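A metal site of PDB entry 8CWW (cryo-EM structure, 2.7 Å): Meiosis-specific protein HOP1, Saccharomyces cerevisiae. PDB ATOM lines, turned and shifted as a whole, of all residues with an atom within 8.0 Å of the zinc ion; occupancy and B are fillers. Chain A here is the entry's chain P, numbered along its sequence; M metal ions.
Within 4 Å of the zinc ion: Cys 14, Cys 16, His 38 and Cys 41.
Along chain A the residues within 4 Å of the zinc ion span positions 14 to 41.
The nearest printed residue that does not touch the zinc ion is Lys 77 (4.6 Å).
The zinc ion is bound by a ring nitrogen (ND1) of His 38 (2.1 Å), the side-chain sulfur of Cys 14 (2.3 Å), the side-chain sulfur of Cys 41 (2.3 Å) and the side-chain sulfur of Cys 16 (2.3 Å).
SG of Cys 14 lies close to OE1 of Glu 15 (3.8 Å).
SG of Cys 16 lies close to NZ of Lys 77, at 3.7 Å.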
ATOM      1  N   SER A  13      28.866  10.960 -22.433  1.00  0.00           N
ATOM      2  CA  SER A  13      27.683  11.528 -23.070  1.00  0.00           C
ATOM      3  C   SER A  13      26.516  10.556 -23.035  1.00  0.00           C
ATOM      4  O   SER A  13      25.359  10.962 -22.970  1.00  0.00           O
ATOM      5  CB  SER A  13      27.997  11.923 -24.517  1.00  0.00           C
ATOM      6  OG  SER A  13      29.066  12.849 -24.572  1.00  0.00           O
ATOM      7  N   CYS A  14      26.833   9.260 -23.082  1.00  0.00           N
ATOM      8  CA  CYS A  14      25.796   8.240 -23.036  1.00  0.00           C
ATOM      9  C   CYS A  14      25.166   8.171 -21.647  1.00  0.00           C
ATOM     10  O   CYS A  14      25.766   8.591 -20.639  1.00  0.00           O
ATOM     11  CB  CYS A  14      26.362   6.872 -23.422  1.00  0.00           C
ATOM     12  SG  CYS A  14      25.121   5.586 -23.682  1.00  0.00           S
ATOM     13  N   GLU A  15      23.944   7.639 -21.596  1.00  0.00           N
ATOM     14  CA  GLU A  15      23.217   7.574 -20.324  1.00  0.00           C
ATOM     15  C   GLU A  15      23.889   6.622 -19.345  1.00  0.00           C
ATOM     16  O   GLU A  15      23.675   6.747 -18.133  1.00  0.00           O
ATOM     17  CB  GLU A  15      21.768   7.154 -20.577  1.00  0.00           C
ATOM     18  CG  GLU A  15      20.897   8.221 -21.223  1.00  0.00           C
ATOM     19  CD  GLU A  15      21.199   8.432 -22.694  1.00  0.00           C
ATOM     20  OE1 GLU A  15      21.972   7.626 -23.265  1.00  0.00           O
ATOM     21  OE2 GLU A  15      20.659   9.392 -23.277  1.00  0.00           O
ATOM     22  N   CYS A  16      24.683   5.669 -19.831  1.00  0.00           N
ATOM     23  CA  CYS A  16      25.385   4.762 -18.925  1.00  0.00           C
ATOM     24  C   CYS A  16      26.398   5.510 -18.084  1.00  0.00           C
ATOM     25  O   CYS A  16      26.610   5.178 -16.908  1.00  0.00           O
ATOM     26  CB  CYS A  16      26.050   3.642 -19.719  1.00  0.00           C
ATOM     27  SG  CYS A  16      27.304   4.180 -20.902  1.00  0.00           S
ATOM     28  N   GLY A  17      27.051   6.521 -18.658  1.00  0.00           N
ATOM     29  CA  GLY A  17      27.941   7.383 -17.921  1.00  0.00           C
ATOM     30  C   GLY A  17      29.354   6.865 -17.731  1.00  0.00           C
ATOM     31  O   GLY A  17      30.179   7.569 -17.132  1.00  0.00           O
ATOM     32  N   LEU A  18      29.652   5.666 -18.216  1.00  0.00           N
ATOM     33  CA  LEU A  18      30.980   5.092 -18.108  1.00  0.00           C
ATOM     34  C   LEU A  18      31.719   5.213 -19.429  1.00  0.00           C
ATOM     35  O   LEU A  18      31.209   5.782 -20.408  1.00  0.00           O
ATOM     36  CB  LEU A  18      30.893   3.626 -17.654  1.00  0.00           C
ATOM     37  CG  LEU A  18      30.378   3.383 -16.239  1.00  0.00           C
ATOM     38  CD1 LEU A  18      30.392   1.899 -15.907  1.00  0.00           C
ATOM     39  CD2 LEU A  18      31.205   4.161 -15.228  1.00  0.00           C
ATOM     40  N   GLU A  19      32.933   4.672 -19.461  1.00  0.00           N
ATOM     41  CA  GLU A  19      33.769   4.687 -20.657  1.00  0.00           C
ATOM     42  C   GLU A  19      33.997   3.259 -21.124  1.00  0.00           C
ATOM     43  O   GLU A  19      34.204   2.352 -20.303  1.00  0.00           O
ATOM     44  CB  GLU A  19      35.111   5.372 -20.382  1.00  0.00           C
ATOM     45  CG  GLU A  19      34.984   6.809 -19.897  1.00  0.00           C
ATOM     46  CD  GLU A  19      34.314   7.711 -20.919  1.00  0.00           C
ATOM     47  OE1 GLU A  19      34.462   7.454 -22.130  1.00  0.00           O
ATOM     48  OE2 GLU A  19      33.644   8.680 -20.507  1.00  0.00           O
ATOM     49  N   VAL A  20      33.953   3.059 -22.431  1.00  0.00           N
ATOM     50  CA  VAL A  20      34.066   1.731 -23.027  1.00  0.00           C
ATOM     51  C   VAL A  20      35.299   1.703 -23.922  1.00  0.00           C
ATOM     52  O   VAL A  20      35.547   2.673 -24.659  1.00  0.00           O
ATOM     53  CB  VAL A  20      32.799   1.357 -23.812  1.00  0.00           C
ATOM     54  CG1 VAL A  20      32.821  -0.106 -24.188  1.00  0.00           C
ATOM     55  CG2 VAL A  20      31.559   1.690 -23.000  1.00  0.00           C
ATOM     56  N   THR A  25      32.885  -1.732 -28.626  1.00  0.00           N
ATOM     57  CA  THR A  25      31.633  -1.250 -29.203  1.00  0.00           C
ATOM     58  C   THR A  25      31.907  -0.399 -30.436  1.00  0.00           C
ATOM     59  O   THR A  25      33.044  -0.184 -30.843  1.00  0.00           O
ATOM     60  CB  THR A  25      30.817  -0.450 -28.180  1.00  0.00           C
ATOM     61  OG1 THR A  25      29.631   0.052 -28.806  1.00  0.00           O
ATOM     62  CG2 THR A  25      31.636   0.719 -27.656  1.00  0.00           C
ATOM     63  N   THR A  36      27.073  11.701 -29.087  1.00  0.00           N
ATOM     64  CA  THR A  36      27.616  10.367 -29.273  1.00  0.00           C
ATOM     65  C   THR A  36      26.924   9.360 -28.347  1.00  0.00           C
ATOM     66  O   THR A  36      26.634   9.659 -27.195  1.00  0.00           O
ATOM     67  CB  THR A  36      29.122  10.365 -29.011  1.00  0.00           C
ATOM     68  OG1 THR A  36      29.749  11.393 -29.781  1.00  0.00           O
ATOM     69  CG2 THR A  36      29.743   9.023 -29.392  1.00  0.00           C
ATOM     70  N   LEU A  37      26.676   8.164 -28.876  1.00  0.00           N
ATOM     71  CA  LEU A  37      26.018   7.106 -28.124  1.00  0.00           C
ATOM     72  C   LEU A  37      26.782   5.811 -28.304  1.00  0.00           C
ATOM     73  O   LEU A  37      27.507   5.624 -29.286  1.00  0.00           O
ATOM     74  CB  LEU A  37      24.559   6.924 -28.568  1.00  0.00           C
ATOM     75  CG  LEU A  37      23.637   8.137 -28.432  1.00  0.00           C
ATOM     76  CD1 LEU A  37      22.246   7.801 -28.936  1.00  0.00           C
ATOM     77  CD2 LEU A  37      23.582   8.614 -26.989  1.00  0.00           C
ATOM     78  N   HIS A  38      26.613   4.911 -27.342  1.00  0.00           N
ATOM     79  CA  HIS A  38      27.234   3.594 -27.392  1.00  0.00           C
ATOM     80  C   HIS A  38      26.376   2.641 -28.212  1.00  0.00           C
ATOM     81  O   HIS A  38      25.151   2.607 -28.064  1.00  0.00           O
ATOM     82  CB  HIS A  38      27.427   3.027 -25.989  1.00  0.00           C
ATOM     83  CG  HIS A  38      28.489   3.711 -25.192  1.00  0.00           C
ATOM     84  ND1 HIS A  38      28.421   3.864 -23.827  1.00  0.00           N
ATOM     85  CD2 HIS A  38      29.658   4.284 -25.568  1.00  0.00           C
ATOM     86  CE1 HIS A  38      29.497   4.498 -23.390  1.00  0.00           C
ATOM     87  NE2 HIS A  38      30.260   4.766 -24.438  1.00  0.00           N
ATOM     88  N   GLY A  39      27.021   1.864 -29.080  1.00  0.00           N
ATOM     89  CA  GLY A  39      26.294   0.879 -29.862  1.00  0.00           C
ATOM     90  C   GLY A  39      25.723  -0.235 -29.015  1.00  0.00           C
ATOM     91  O   GLY A  39      24.567  -0.642 -29.210  1.00  0.00           O
ATOM     92  N   ILE A  40      26.508  -0.753 -28.066  1.00  0.00           N
ATOM     93  CA  ILE A  40      26.037  -1.846 -27.220  1.00  0.00           C
ATOM     94  C   ILE A  40      24.915  -1.408 -26.295  1.00  0.00           C
ATOM     95  O   ILE A  40      24.092  -2.247 -25.907  1.00  0.00           O
ATOM     96  CB  ILE A  40      27.210  -2.435 -26.421  1.00  0.00           C
ATOM     97  CG1 ILE A  40      27.872  -1.354 -25.559  1.00  0.00           C
ATOM     98  CG2 ILE A  40      28.232  -3.063 -27.349  1.00  0.00           C
ATOM     99  CD1 ILE A  40      29.097  -1.840 -24.822  1.00  0.00           C
ATOM    100  N   CYS A  41      24.857  -0.134 -25.924  1.00  0.00           N
ATOM    101  CA  CYS A  41      23.775   0.353 -25.071  1.00  0.00           C
ATOM    102  C   CYS A  41      22.440   0.432 -25.791  1.00  0.00           C
ATOM    103  O   CYS A  41      21.414   0.601 -25.127  1.00  0.00           O
ATOM    104  CB  CYS A  41      24.139   1.736 -24.508  1.00  0.00           C
ATOM    105  SG  CYS A  41      25.503   1.747 -23.317  1.00  0.00           S
ATOM    106  N   TYR A  42      22.414   0.320 -27.115  1.00  0.00           N
ATOM    107  CA  TYR A  42      21.182   0.473 -27.888  1.00  0.00           C
ATOM    108  C   TYR A  42      20.847  -0.752 -28.727  1.00  0.00           C
ATOM    109  O   TYR A  42      19.890  -0.692 -29.511  1.00  0.00           O
ATOM    110  CB  TYR A  42      21.252   1.719 -28.775  1.00  0.00           C
ATOM    111  CG  TYR A  42      21.047   3.011 -28.012  1.00  0.00           C
ATOM    112  CD1 TYR A  42      22.132   3.714 -27.503  1.00  0.00           C
ATOM    113  CD2 TYR A  42      19.774   3.507 -27.798  1.00  0.00           C
ATOM    114  CE1 TYR A  42      21.946   4.884 -26.810  1.00  0.00           C
ATOM    115  CE2 TYR A  42      19.585   4.681 -27.097  1.00  0.00           C
ATOM    116  CZ  TYR A  42      20.675   5.375 -26.605  1.00  0.00           C
ATOM    117  OH  TYR A  42      20.479   6.542 -25.914  1.00  0.00           O
ATOM    118  N   MET A  73      20.993  -0.326 -17.653  1.00  0.00           N
ATOM    119  CA  MET A  73      22.075  -0.076 -18.607  1.00  0.00           C
ATOM    120  C   MET A  73      23.143  -1.161 -18.525  1.00  0.00           C
ATOM    121  O   MET A  73      23.624  -1.630 -19.555  1.00  0.00           O
ATOM    122  CB  MET A  73      22.696   1.300 -18.357  1.00  0.00           C
ATOM    123  CG  MET A  73      21.776   2.479 -18.666  1.00  0.00           C
ATOM    124  SD  MET A  73      21.281   2.559 -20.394  1.00  0.00           S
ATOM    125  CE  MET A  73      19.600   1.945 -20.301  1.00  0.00           C
ATOM    126  N   LYS A  77      24.122  -3.687 -21.514  1.00  0.00           N
ATOM    127  CA  LYS A  77      25.510  -3.644 -21.956  1.00  0.00           C
ATOM    128  C   LYS A  77      26.113  -5.037 -22.007  1.00  0.00           C
ATOM    129  O   LYS A  77      26.698  -5.446 -23.011  1.00  0.00           O
ATOM    130  CB  LYS A  77      26.310  -2.744 -21.009  1.00  0.00           C
ATOM    131  CG  LYS A  77      27.200  -1.723 -21.686  1.00  0.00           C
ATOM    132  CD  LYS A  77      27.873  -0.848 -20.638  1.00  0.00           C
ATOM    133  CE  LYS A  77      28.698   0.256 -21.274  1.00  0.00           C
ATOM    134  NZ  LYS A  77      29.332   1.128 -20.238  1.00  0.00           N
HETATM  135 ZN    ZN M   1      26.495   3.830 -23.050  1.00  0.00          ZN
